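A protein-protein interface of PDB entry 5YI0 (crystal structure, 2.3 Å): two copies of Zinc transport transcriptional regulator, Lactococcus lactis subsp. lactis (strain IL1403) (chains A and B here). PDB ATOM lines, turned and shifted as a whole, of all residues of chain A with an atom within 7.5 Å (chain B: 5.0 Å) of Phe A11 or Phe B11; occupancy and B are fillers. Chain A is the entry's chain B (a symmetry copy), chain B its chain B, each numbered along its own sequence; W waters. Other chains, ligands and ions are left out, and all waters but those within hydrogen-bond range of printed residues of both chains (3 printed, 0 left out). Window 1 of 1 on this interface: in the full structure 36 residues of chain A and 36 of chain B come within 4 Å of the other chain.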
ATOM      1  N   GLY A   1     -27.444  -0.716  -0.961  1.00  0.00           N
ATOM      2  CA  GLY A   1     -28.565  -0.012  -0.372  1.00  0.00           C
ATOM      3  C   GLY A   1     -28.105   0.296   1.022  1.00  0.00           C
ATOM      4  O   GLY A   1     -27.137  -0.320   1.443  1.00  0.00           O
ATOM      5  N   LEU A   4     -27.835  -2.872   6.033  1.00  0.00           N
ATOM      6  CA  LEU A   4     -26.823  -3.897   5.811  1.00  0.00           C
ATOM      7  C   LEU A   4     -27.408  -5.031   4.973  1.00  0.00           C
ATOM      8  O   LEU A   4     -26.760  -5.542   4.059  1.00  0.00           O
ATOM      9  CB  LEU A   4     -26.259  -4.428   7.134  1.00  0.00           C
ATOM     10  CG  LEU A   4     -25.031  -5.348   7.025  1.00  0.00           C
ATOM     11  CD1 LEU A   4     -23.796  -4.592   6.595  1.00  0.00           C
ATOM     12  CD2 LEU A   4     -24.760  -6.003   8.344  1.00  0.00           C
ATOM     13  N   ALA A   5     -28.647  -5.410   5.259  1.00  0.00           N
ATOM     14  CA  ALA A   5     -29.297  -6.452   4.475  1.00  0.00           C
ATOM     15  C   ALA A   5     -29.260  -6.070   2.999  1.00  0.00           C
ATOM     16  O   ALA A   5     -28.884  -6.876   2.144  1.00  0.00           O
ATOM     17  CB  ALA A   5     -30.734  -6.681   4.945  1.00  0.00           C
ATOM     18  N   ASN A   6     -29.622  -4.828   2.690  1.00  0.00           N
ATOM     19  CA  ASN A   6     -29.578  -4.384   1.300  1.00  0.00           C
ATOM     20  C   ASN A   6     -28.152  -4.343   0.751  1.00  0.00           C
ATOM     21  O   ASN A   6     -27.918  -4.651  -0.414  1.00  0.00           O
ATOM     22  CB  ASN A   6     -30.226  -3.019   1.134  1.00  0.00           C
ATOM     23  CG  ASN A   6     -31.733  -3.087   1.164  1.00  0.00           C
ATOM     24  OD1 ASN A   6     -32.381  -2.291   1.843  1.00  0.00           O
ATOM     25  ND2 ASN A   6     -32.305  -4.039   0.422  1.00  0.00           N
ATOM     26  N   GLN A   7     -27.199  -3.969   1.589  1.00  0.00           N
ATOM     27  CA  GLN A   7     -25.831  -3.931   1.132  1.00  0.00           C
ATOM     28  C   GLN A   7     -25.358  -5.355   0.849  1.00  0.00           C
ATOM     29  O   GLN A   7     -24.715  -5.625  -0.175  1.00  0.00           O
ATOM     30  CB  GLN A   7     -24.934  -3.256   2.159  1.00  0.00           C
ATOM     31  CG  GLN A   7     -23.504  -3.151   1.679  1.00  0.00           C
ATOM     32  CD  GLN A   7     -22.627  -2.310   2.579  1.00  0.00           C
ATOM     33  OE1 GLN A   7     -23.029  -1.905   3.686  1.00  0.00           O
ATOM     34  NE2 GLN A   7     -21.417  -2.032   2.108  1.00  0.00           N
ATOM     35  N   ILE A   8     -25.699  -6.278   1.742  1.00  0.00           N
ATOM     36  CA  ILE A   8     -25.324  -7.675   1.545  1.00  0.00           C
ATOM     37  C   ILE A   8     -25.918  -8.188   0.237  1.00  0.00           C
ATOM     38  O   ILE A   8     -25.211  -8.741  -0.616  1.00  0.00           O
ATOM     39  CB  ILE A   8     -25.769  -8.532   2.746  1.00  0.00           C
ATOM     40  CG1 ILE A   8     -24.881  -8.215   3.964  1.00  0.00           C
ATOM     41  CG2 ILE A   8     -25.749  -9.983   2.368  1.00  0.00           C
ATOM     42  CD1 ILE A   8     -25.502  -8.569   5.268  1.00  0.00           C
ATOM     43  N   ASP A   9     -27.212  -7.957   0.049  1.00  0.00           N
ATOM     44  CA  ASP A   9     -27.872  -8.316  -1.224  1.00  0.00           C
ATOM     45  C   ASP A   9     -27.188  -7.706  -2.457  1.00  0.00           C
ATOM     46  O   ASP A   9     -26.919  -8.399  -3.439  1.00  0.00           O
ATOM     47  CB  ASP A   9     -29.364  -7.988  -1.166  1.00  0.00           C
ATOM     48  CG  ASP A   9     -30.120  -8.450  -2.396  1.00  0.00           C
ATOM     49  OD1 ASP A   9     -30.324  -9.664  -2.597  1.00  0.00           O
ATOM     50  OD2 ASP A   9     -30.537  -7.580  -3.169  1.00  0.00           O
ATOM     51  N   GLN A  10     -26.848  -6.427  -2.412  1.00  0.00           N
ATOM     52  CA  GLN A  10     -26.156  -5.834  -3.569  1.00  0.00           C
ATOM     53  C   GLN A  10     -24.774  -6.416  -3.815  1.00  0.00           C
ATOM     54  O   GLN A  10     -24.353  -6.548  -4.953  1.00  0.00           O
ATOM     55  CB  GLN A  10     -26.025  -4.331  -3.407  1.00  0.00           C
ATOM     56  CG  GLN A  10     -27.343  -3.627  -3.275  1.00  0.00           C
ATOM     57  CD  GLN A  10     -27.287  -2.216  -3.825  1.00  0.00           C
ATOM     58  OE1 GLN A  10     -26.516  -1.373  -3.344  1.00  0.00           O
ATOM     59  NE2 GLN A  10     -28.087  -1.955  -4.861  1.00  0.00           N
ATOM     60  N   PHE A  11     -24.065  -6.733  -2.731  1.00  0.00           N
ATOM     61  CA  PHE A  11     -22.725  -7.278  -2.830  1.00  0.00           C
ATOM     62  C   PHE A  11     -22.741  -8.661  -3.497  1.00  0.00           C
ATOM     63  O   PHE A  11     -21.973  -8.919  -4.435  1.00  0.00           O
ATOM     64  CB  PHE A  11     -22.058  -7.337  -1.452  1.00  0.00           C
ATOM     65  CG  PHE A  11     -20.859  -8.227  -1.405  1.00  0.00           C
ATOM     66  CD1 PHE A  11     -19.653  -7.804  -1.921  1.00  0.00           C
ATOM     67  CD2 PHE A  11     -20.939  -9.493  -0.868  1.00  0.00           C
ATOM     68  CE1 PHE A  11     -18.527  -8.611  -1.876  1.00  0.00           C
ATOM     69  CE2 PHE A  11     -19.812 -10.317  -0.825  1.00  0.00           C
ATOM     70  CZ  PHE A  11     -18.602  -9.865  -1.338  1.00  0.00           C
ATOM     71  N   LEU A  12     -23.627  -9.537  -3.048  1.00  0.00           N
ATOM     72  CA  LEU A  12     -23.840 -10.815  -3.774  1.00  0.00           C
ATOM     73  C   LEU A  12     -24.202 -10.636  -5.264  1.00  0.00           C
ATOM     74  O   LEU A  12     -23.719 -11.373  -6.140  1.00  0.00           O
ATOM     75  CB  LEU A  12     -24.878 -11.688  -3.067  1.00  0.00           C
ATOM     76  CG  LEU A  12     -24.460 -11.923  -1.604  1.00  0.00           C
ATOM     77  CD1 LEU A  12     -25.427 -12.832  -0.883  1.00  0.00           C
ATOM     78  CD2 LEU A  12     -23.033 -12.475  -1.525  1.00  0.00           C
ATOM     79  N   GLY A  13     -25.043  -9.653  -5.549  1.00  0.00           N
ATOM     80  CA  GLY A  13     -25.405  -9.362  -6.925  1.00  0.00           C
ATOM     81  C   GLY A  13     -24.149  -9.040  -7.710  1.00  0.00           C
ATOM     82  O   GLY A  13     -23.944  -9.559  -8.806  1.00  0.00           O
ATOM     83  N   THR A  14     -23.292  -8.196  -7.131  1.00  0.00           N
ATOM     84  CA  THR A  14     -22.037  -7.807  -7.772  1.00  0.00           C
ATOM     85  C   THR A  14     -21.155  -9.004  -8.081  1.00  0.00           C
ATOM     86  O   THR A  14     -20.508  -9.060  -9.121  1.00  0.00           O
ATOM     87  CB  THR A  14     -21.263  -6.821  -6.901  1.00  0.00           C
ATOM     88  OG1 THR A  14     -22.039  -5.633  -6.752  1.00  0.00           O
ATOM     89  CG2 THR A  14     -19.926  -6.465  -7.532  1.00  0.00           C
ATOM     90  N   ILE A  15     -21.125  -9.962  -7.163  1.00  0.00           N
ATOM     91  CA  ILE A  15     -20.253 -11.112  -7.317  1.00  0.00           C
ATOM     92  C   ILE A  15     -20.831 -12.016  -8.398  1.00  0.00           C
ATOM     93  O   ILE A  15     -20.113 -12.533  -9.250  1.00  0.00           O
ATOM     94  CB  ILE A  15     -20.065 -11.849  -5.963  1.00  0.00           C
ATOM     95  CG1 ILE A  15     -19.298 -10.947  -4.991  1.00  0.00           C
ATOM     96  CG2 ILE A  15     -19.337 -13.175  -6.148  1.00  0.00           C
ATOM     97  CD1 ILE A  15     -17.963 -10.500  -5.531  1.00  0.00           C
ATOM     98  N   MET A  16     -22.148 -12.174  -8.374  1.00  0.00           N
ATOM     99  CA  MET A  16     -22.830 -12.958  -9.390  1.00  0.00           C
ATOM    100  C   MET A  16     -22.536 -12.451 -10.817  1.00  0.00           C
ATOM    101  O   MET A  16     -22.094 -13.216 -11.675  1.00  0.00           O
ATOM    102  CB  MET A  16     -24.337 -13.016  -9.134  1.00  0.00           C
ATOM    103  CG  MET A  16     -25.016 -14.143  -9.902  1.00  0.00           C
ATOM    104  SD  MET A  16     -26.797 -13.964 -10.017  1.00  0.00           S
ATOM    105  CE  MET A  16     -27.290 -15.645 -10.401  1.00  0.00           C
ATOM    106  N   GLN A  17     -22.765 -11.172 -11.070  1.00  0.00           N
ATOM    107  CA  GLN A  17     -22.422 -10.605 -12.371  1.00  0.00           C
ATOM    108  C   GLN A  17     -20.952 -10.839 -12.734  1.00  0.00           C
ATOM    109  O   GLN A  17     -20.635 -11.097 -13.889  1.00  0.00           O
ATOM    110  CB  GLN A  17     -22.747  -9.111 -12.432  1.00  0.00           C
ATOM    111  CG  GLN A  17     -22.196  -8.392 -13.667  1.00  0.00           C
ATOM    112  CD  GLN A  17     -23.098  -8.527 -14.895  1.00  0.00           C
ATOM    113  OE1 GLN A  17     -24.326  -8.408 -14.794  1.00  0.00           O
ATOM    114  NE2 GLN A  17     -22.490  -8.772 -16.062  1.00  0.00           N
ATOM    115  N   ILE A  25     -13.342 -17.461  -9.377  1.00  0.00           N
ATOM    116  CA  ILE A  25     -13.338 -16.042  -9.005  1.00  0.00           C
ATOM    117  C   ILE A  25     -11.908 -15.562  -8.845  1.00  0.00           C
ATOM    118  O   ILE A  25     -11.265 -15.837  -7.832  1.00  0.00           O
ATOM    119  CB  ILE A  25     -14.088 -15.771  -7.690  1.00  0.00           C
ATOM    120  CG1 ILE A  25     -15.535 -16.295  -7.749  1.00  0.00           C
ATOM    121  CG2 ILE A  25     -14.028 -14.285  -7.355  1.00  0.00           C
ATOM    122  CD1 ILE A  25     -16.528 -15.379  -8.418  1.00  0.00           C
ATOM    123  N   PHE A 137     -19.017 -13.098  10.474  1.00  0.00           N
ATOM    124  CA  PHE A 137     -19.948 -12.747   9.408  1.00  0.00           C
ATOM    125  C   PHE A 137     -19.817 -13.668   8.175  1.00  0.00           C
ATOM    126  O   PHE A 137     -20.804 -14.128   7.611  1.00  0.00           O
ATOM    127  CB  PHE A 137     -19.773 -11.269   9.003  1.00  0.00           C
ATOM    128  CG  PHE A 137     -20.546 -10.900   7.788  1.00  0.00           C
ATOM    129  CD1 PHE A 137     -21.909 -10.725   7.860  1.00  0.00           C
ATOM    130  CD2 PHE A 137     -19.917 -10.771   6.560  1.00  0.00           C
ATOM    131  CE1 PHE A 137     -22.643 -10.418   6.741  1.00  0.00           C
ATOM    132  CE2 PHE A 137     -20.639 -10.472   5.432  1.00  0.00           C
ATOM    133  CZ  PHE A 137     -21.998 -10.289   5.517  1.00  0.00           C
ATOM    134  N   LEU A 138     -18.607 -13.941   7.723  1.00  0.00           N
ATOM    135  CA  LEU A 138     -18.486 -14.775   6.519  1.00  0.00           C
ATOM    136  C   LEU A 138     -18.889 -16.246   6.761  1.00  0.00           C
ATOM    137  O   LEU A 138     -19.525 -16.860   5.918  1.00  0.00           O
ATOM    138  CB  LEU A 138     -17.085 -14.678   5.911  1.00  0.00           C
ATOM    139  CG  LEU A 138     -16.701 -13.285   5.410  1.00  0.00           C
ATOM    140  CD1 LEU A 138     -15.239 -13.232   5.086  1.00  0.00           C
ATOM    141  CD2 LEU A 138     -17.536 -12.860   4.191  1.00  0.00           C
ATOM    142  N   SER A 139     -18.527 -16.802   7.911  1.00  0.00           N
ATOM    143  CA  SER A 139     -18.912 -18.176   8.242  1.00  0.00           C
ATOM    144  C   SER A 139     -20.426 -18.328   8.268  1.00  0.00           C
ATOM    145  O   SER A 139     -20.972 -19.274   7.698  1.00  0.00           O
ATOM    146  CB  SER A 139     -18.358 -18.583   9.611  1.00  0.00           C
ATOM    147  OG  SER A 139     -16.944 -18.621   9.591  1.00  0.00           O
ATOM    148  N   ALA A 140     -21.101 -17.390   8.927  1.00  0.00           N
ATOM    149  CA  ALA A 140     -22.540 -17.474   9.077  1.00  0.00           C
ATOM    150  C   ALA A 140     -23.230 -17.309   7.726  1.00  0.00           C
ATOM    151  O   ALA A 140     -24.216 -17.979   7.446  1.00  0.00           O
ATOM    152  CB  ALA A 140     -23.032 -16.410  10.076  1.00  0.00           C
ATOM    153  N   LEU A 141     -22.706 -16.426   6.879  1.00  0.00           N
ATOM    154  CA  LEU A 141     -23.348 -16.162   5.589  1.00  0.00           C
ATOM    155  C   LEU A 141     -23.049 -17.341   4.653  1.00  0.00           C
ATOM    156  O   LEU A 141     -23.879 -17.744   3.810  1.00  0.00           O
ATOM    157  CB  LEU A 141     -22.862 -14.803   5.013  1.00  0.00           C
ATOM    158  CG  LEU A 141     -23.403 -14.295   3.665  1.00  0.00           C
ATOM    159  CD1 LEU A 141     -24.911 -14.147   3.704  1.00  0.00           C
ATOM    160  CD2 LEU A 141     -22.751 -12.982   3.176  1.00  0.00           C
ATOM    161  N   THR A 142     -21.863 -17.912   4.822  1.00  0.00           N
ATOM    162  CA  THR A 142     -21.482 -19.159   4.132  1.00  0.00           C
ATOM    163  C   THR A 142     -22.468 -20.297   4.408  1.00  0.00           C
ATOM    164  O   THR A 142     -22.757 -21.110   3.532  1.00  0.00           O
ATOM    165  CB  THR A 142     -20.070 -19.630   4.551  1.00  0.00           C
ATOM    166  OG1 THR A 142     -19.074 -18.727   4.020  1.00  0.00           O
ATOM    167  CG2 THR A 142     -19.800 -21.051   4.048  1.00  0.00           C
ATOM    168  N   GLU A 143     -22.984 -20.360   5.632  1.00  0.00           N
ATOM    169  CA  GLU A 143     -23.883 -21.454   6.017  1.00  0.00           C
ATOM    170  C   GLU A 143     -25.211 -21.369   5.273  1.00  0.00           C
ATOM    171  O   GLU A 143     -25.834 -22.382   4.999  1.00  0.00           O
ATOM    172  CB  GLU A 143     -24.156 -21.428   7.517  1.00  0.00           C
ATOM    173  CG  GLU A 143     -23.045 -21.964   8.365  1.00  0.00           C
ATOM    174  CD  GLU A 143     -23.268 -21.662   9.828  1.00  0.00           C
ATOM    175  OE1 GLU A 143     -24.290 -22.112  10.393  1.00  0.00           O
ATOM    176  OE2 GLU A 143     -22.423 -20.950  10.402  1.00  0.00           O
ATOM    177  N   PHE A 145     -25.661 -20.583   2.320  1.00  0.00           N
ATOM    178  CA  PHE A 145     -25.563 -20.944   0.921  1.00  0.00           C
ATOM    179  C   PHE A 145     -25.323 -22.437   0.643  1.00  0.00           C
ATOM    180  O   PHE A 145     -24.683 -22.805  -0.338  1.00  0.00           O
ATOM    181  CB  PHE A 145     -24.576 -20.018   0.215  1.00  0.00           C
ATOM    182  CG  PHE A 145     -25.135 -18.650  -0.005  1.00  0.00           C
ATOM    183  CD1 PHE A 145     -26.044 -18.424  -1.035  1.00  0.00           C
ATOM    184  CD2 PHE A 145     -24.820 -17.613   0.840  1.00  0.00           C
ATOM    185  CE1 PHE A 145     -26.596 -17.195  -1.219  1.00  0.00           C
ATOM    186  CE2 PHE A 145     -25.360 -16.370   0.654  1.00  0.00           C
ATOM    187  CZ  PHE A 145     -26.250 -16.156  -0.376  1.00  0.00           C
ATOM    188  N   ASN B   6      -7.654 -16.353   2.889  1.00  0.00           N
ATOM    189  CA  ASN B   6      -8.136 -17.663   2.464  1.00  0.00           C
ATOM    190  C   ASN B   6      -9.632 -17.842   2.724  1.00  0.00           C
ATOM    191  O   ASN B   6     -10.336 -18.466   1.937  1.00  0.00           O
ATOM    192  CB  ASN B   6      -7.364 -18.785   3.142  1.00  0.00           C
ATOM    193  CG  ASN B   6      -5.994 -18.988   2.542  1.00  0.00           C
ATOM    194  OD1 ASN B   6      -5.008 -19.114   3.267  1.00  0.00           O
ATOM    195  ND2 ASN B   6      -5.923 -19.027   1.209  1.00  0.00           N
ATOM    196  N   GLN B   7     -10.117 -17.292   3.825  1.00  0.00           N
ATOM    197  CA  GLN B   7     -11.525 -17.411   4.113  1.00  0.00           C
ATOM    198  C   GLN B   7     -12.317 -16.616   3.076  1.00  0.00           C
ATOM    199  O   GLN B   7     -13.335 -17.086   2.548  1.00  0.00           O
ATOM    200  CB  GLN B   7     -11.835 -16.923   5.521  1.00  0.00           C
ATOM    201  CG  GLN B   7     -13.297 -17.091   5.869  1.00  0.00           C
ATOM    202  CD  GLN B   7     -13.606 -16.810   7.322  1.00  0.00           C
ATOM    203  OE1 GLN B   7     -12.753 -16.322   8.086  1.00  0.00           O
ATOM    204  NE2 GLN B   7     -14.834 -17.123   7.720  1.00  0.00           N
ATOM    205  N   ILE B   8     -11.836 -15.418   2.759  1.00  0.00           N
ATOM    206  CA  ILE B   8     -12.502 -14.595   1.754  1.00  0.00           C
ATOM    207  C   ILE B   8     -12.545 -15.341   0.424  1.00  0.00           C
ATOM    208  O   ILE B   8     -13.607 -15.490  -0.195  1.00  0.00           O
ATOM    209  CB  ILE B   8     -11.800 -13.229   1.618  1.00  0.00           C
ATOM    210  CG1 ILE B   8     -12.094 -12.371   2.862  1.00  0.00           C
ATOM    211  CG2 ILE B   8     -12.220 -12.569   0.338  1.00  0.00           C
ATOM    212  CD1 ILE B   8     -11.104 -11.287   3.091  1.00  0.00           C
ATOM    213  N   ASP B   9     -11.397 -15.862   0.005  1.00  0.00           N
ATOM    214  CA  ASP B   9     -11.338 -16.692  -1.216  1.00  0.00           C
ATOM    215  C   ASP B   9     -12.314 -17.879  -1.191  1.00  0.00           C
ATOM    216  O   ASP B   9     -13.051 -18.112  -2.150  1.00  0.00           O
ATOM    217  CB  ASP B   9      -9.900 -17.128  -1.500  1.00  0.00           C
ATOM    218  CG  ASP B   9      -9.757 -17.878  -2.810  1.00  0.00           C
ATOM    219  OD1 ASP B   9      -9.865 -17.280  -3.899  1.00  0.00           O
ATOM    220  OD2 ASP B   9      -9.512 -19.088  -2.749  1.00  0.00           O
ATOM    221  N   GLN B  10     -12.377 -18.610  -0.090  1.00  0.00           N
ATOM    222  CA  GLN B  10     -13.335 -19.728  -0.032  1.00  0.00           C
ATOM    223  C   GLN B  10     -14.788 -19.287  -0.082  1.00  0.00           C
ATOM    224  O   GLN B  10     -15.621 -19.972  -0.654  1.00  0.00           O
ATOM    225  CB  GLN B  10     -13.124 -20.556   1.223  1.00  0.00           C
ATOM    226  CG  GLN B  10     -11.749 -21.148   1.324  1.00  0.00           C
ATOM    227  CD  GLN B  10     -11.754 -22.457   2.086  1.00  0.00           C
ATOM    228  OE1 GLN B  10     -12.124 -22.507   3.269  1.00  0.00           O
ATOM    229  NE2 GLN B  10     -11.369 -23.538   1.405  1.00  0.00           N
ATOM    230  N   PHE B  11     -15.083 -18.151   0.550  1.00  0.00           N
ATOM    231  CA  PHE B  11     -16.437 -17.632   0.594  1.00  0.00           C
ATOM    232  C   PHE B  11     -16.920 -17.237  -0.809  1.00  0.00           C
ATOM    233  O   PHE B  11     -18.016 -17.630  -1.233  1.00  0.00           O
ATOM    234  CB  PHE B  11     -16.536 -16.452   1.565  1.00  0.00           C
ATOM    235  CG  PHE B  11     -17.768 -15.628   1.381  1.00  0.00           C
ATOM    236  CD1 PHE B  11     -18.983 -16.068   1.861  1.00  0.00           C
ATOM    237  CD2 PHE B  11     -17.721 -14.426   0.710  1.00  0.00           C
ATOM    238  CE1 PHE B  11     -20.135 -15.312   1.709  1.00  0.00           C
ATOM    239  CE2 PHE B  11     -18.877 -13.661   0.545  1.00  0.00           C
ATOM    240  CZ  PHE B  11     -20.089 -14.117   1.050  1.00  0.00           C
ATOM    241  N   LEU B  12     -16.102 -16.497  -1.542  1.00  0.00           N
ATOM    242  CA  LEU B  12     -16.410 -16.248  -2.973  1.00  0.00           C
ATOM    243  C   LEU B  12     -16.607 -17.535  -3.804  1.00  0.00           C
ATOM    244  O   LEU B  12     -17.508 -17.623  -4.656  1.00  0.00           O
ATOM    245  CB  LEU B  12     -15.356 -15.346  -3.619  1.00  0.00           C
ATOM    246  CG  LEU B  12     -15.230 -14.034  -2.823  1.00  0.00           C
ATOM    247  CD1 LEU B  12     -14.242 -13.085  -3.460  1.00  0.00           C
ATOM    248  CD2 LEU B  12     -16.597 -13.363  -2.654  1.00  0.00           C
ATOM    249  N   GLY B  13     -15.773 -18.532  -3.548  1.00  0.00           N
ATOM    250  CA  GLY B  13     -15.909 -19.806  -4.233  1.00  0.00           C
ATOM    251  C   GLY B  13     -17.288 -20.371  -3.958  1.00  0.00           C
ATOM    252  O   GLY B  13     -17.978 -20.813  -4.875  1.00  0.00           O
ATOM    253  N   THR B  14     -17.698 -20.333  -2.689  1.00  0.00           N
ATOM    254  CA  THR B  14     -19.011 -20.836  -2.285  1.00  0.00           C
ATOM    255  C   THR B  14     -20.143 -20.134  -3.014  1.00  0.00           C
ATOM    256  O   THR B  14     -21.132 -20.754  -3.390  1.00  0.00           O
ATOM    257  CB  THR B  14     -19.212 -20.687  -0.779  1.00  0.00           C
ATOM    258  OG1 THR B  14     -18.238 -21.484  -0.106  1.00  0.00           O
ATOM    259  CG2 THR B  14     -20.600 -21.146  -0.364  1.00  0.00           C
ATOM    260  N   ILE B  15     -19.998 -18.829  -3.204  1.00  0.00           N
ATOM    261  CA  ILE B  15     -21.055 -18.044  -3.815  1.00  0.00           C
ATOM    262  C   ILE B  15     -21.096 -18.366  -5.304  1.00  0.00           C
ATOM    263  O   ILE B  15     -22.162 -18.536  -5.891  1.00  0.00           O
ATOM    264  CB  ILE B  15     -20.849 -16.530  -3.541  1.00  0.00           C
ATOM    265  CG1 ILE B  15     -21.021 -16.254  -2.043  1.00  0.00           C
ATOM    266  CG2 ILE B  15     -21.819 -15.680  -4.354  1.00  0.00           C
ATOM    267  CD1 ILE B  15     -22.357 -16.704  -1.510  1.00  0.00           C
ATOM    268  N   LEU B 138     -17.415  -4.760   3.054  1.00  0.00           N
ATOM    269  CA  LEU B 138     -18.126  -5.094   1.812  1.00  0.00           C
ATOM    270  C   LEU B 138     -17.932  -4.036   0.704  1.00  0.00           C
ATOM    271  O   LEU B 138     -17.780  -4.379  -0.458  1.00  0.00           O
ATOM    272  CB  LEU B 138     -19.610  -5.356   2.072  1.00  0.00           C
ATOM    273  CG  LEU B 138     -19.899  -6.559   2.972  1.00  0.00           C
ATOM    274  CD1 LEU B 138     -21.341  -6.572   3.380  1.00  0.00           C
ATOM    275  CD2 LEU B 138     -19.520  -7.888   2.297  1.00  0.00           C
ATOM    276  N   LEU B 141     -14.448  -4.515  -0.797  1.00  0.00           N
ATOM    277  CA  LEU B 141     -14.301  -5.759  -1.558  1.00  0.00           C
ATOM    278  C   LEU B 141     -15.136  -5.638  -2.841  1.00  0.00           C
ATOM    279  O   LEU B 141     -14.769  -6.152  -3.919  1.00  0.00           O
ATOM    280  CB  LEU B 141     -14.716  -6.977  -0.687  1.00  0.00           C
ATOM    281  CG  LEU B 141     -14.639  -8.402  -1.261  1.00  0.00           C
ATOM    282  CD1 LEU B 141     -13.226  -8.739  -1.696  1.00  0.00           C
ATOM    283  CD2 LEU B 141     -15.180  -9.496  -0.313  1.00  0.00           C
ATOM    284  N   THR B 142     -16.253  -4.931  -2.725  1.00  0.00           N
ATOM    285  CA  THR B 142     -17.082  -4.571  -3.891  1.00  0.00           C
ATOM    286  C   THR B 142     -16.285  -3.806  -4.952  1.00  0.00           C
ATOM    287  O   THR B 142     -16.497  -3.983  -6.151  1.00  0.00           O
ATOM    288  CB  THR B 142     -18.293  -3.702  -3.478  1.00  0.00           C
ATOM    289  OG1 THR B 142     -19.236  -4.501  -2.729  1.00  0.00           O
ATOM    290  CG2 THR B 142     -18.981  -3.109  -4.711  1.00  0.00           C
HETATM  291  O   HOH W   1     -20.981  -3.050  -0.806  1.00  0.00           O
HETATM  292  O   HOH W   2     -11.452 -15.472  -5.225  1.00  0.00           O
HETATM  293  O   HOH W   3     -16.506 -18.549   5.510  1.00  0.00           O
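The side-chain amide nitrogen (NE2) of Gln B7 lies within hydrogen-bond range of the side-chain hydroxyl (OG) of Ser A139 (3.2 Å).
O of Leu B138 is in hydrogen-bond range of OG1 of Thr B142 (2.7 Å).
O of Leu A138 sits at hydrogen-bond distance from OG1 of Thr A142 (2.7 Å).
Gln A7 touches Leu B138 (NE2 to CB, 3.8 Å).
CD1 of Leu B138 touches CG1 of Ile A8, 3.9 Å away.
Phe B11 touches Phe A11 (CE2 to CE2, 3.7 Å).
Phe A11 touches Leu B138 (CD2 to CD2, 3.8 Å).
Phe A11 touches Leu B141 (CZ to CD2, 3.6 Å).
Ile B15 touches Ile A15.
Ile A25 touches Leu B12 (CG1 to O, 3.9 Å).
Leu A138 touches Ile B8.
CD2 of Phe B11 touches CD2 of Leu A138, 3.8 Å away.
Leu A141 touches Phe B11 (CD2 to CZ, 3.6 Å).
Of chain B, only Phe B11 (3.7 Å), Leu B138 (3.8 Å), Leu B141 (3.6 Å) and Thr B142 (3.4 Å) come within 4 Å of Phe A11.
Phe B11 touches four residues of chain A.
Printed residues of chain B within 4 Å of Ile A8: Leu B138.
Printed residues of chain B within 4 Å of Ser A139: Gln B7 (3.2 Å).
Printed residues of chain B within 4 Å of Leu A138: Gln B7 (3.8 Å), Ile B8 (3.9 Å) and Phe B11 (3.8 Å).
Of the printed residues of chain A, Leu B141 touches Phe A11.
Asn B6 touches none of the printed residues of chain A.
Leu A12 touches none of the printed residues of chain B.
The nearest residue of chain B that does not touch Phe A11 is Leu B12 (4.2 Å).
The nearest residue of chain A that does not touch Phe B11 is Leu A12 (4.2 Å).
The nearest printed residue of chain B that does not touch Ile A8 is Phe B11 (7.1 Å).
Hydrophobic or aromatic side chains of chain A that line the printed part of chain B: Ile A8, Phe A11, Ile A15, Ile A25, Leu A138, Leu A141 and Phe A145.
Hydrophobic or aromatic side chains of chain B within 4 Å of the printed part of chain A: Ile B8, Phe B11, Ile B15, Leu B138 and Leu B141.
Among the printed residues, no Asp or Glu carboxylate lies within 4 Å of a Lys or Arg side-chain nitrogen of the other chain.
Ile A8 touches Leu B138, and with the chains exchanged Leu A138 touches Ile B8.
Phe A11 touches its own counterpart, Phe B11.
Phe A11 touches Leu B138, and with the chains exchanged Leu A138 touches Phe B11.
Phe A11 touches Leu B141, and with the chains exchanged Leu A141 touches Phe B11.
13 positions are printed for both chains.
Of the 15 pairs that touch across the chains among the printed residues, 12 have their exchanged pair printed and touching as well.
Water W2 bridges the backbone carbonyl oxygen of Ile A25 (2.6 Å) and the side-chain carboxylate of Asp B9 (2.7 Å).
Water W1 lies within hydrogen-bond range of the side-chain hydroxyl of Thr B142 (3.0 Å), the side-chain amide nitrogen of Gln A7 (3.1 Å) and the backbone carbonyl oxygen of Leu B138 (3.5 Å).
Water W3 lies within hydrogen-bond range of OG1 of Thr A142, NE2 of Gln B7 and O of Leu A138.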
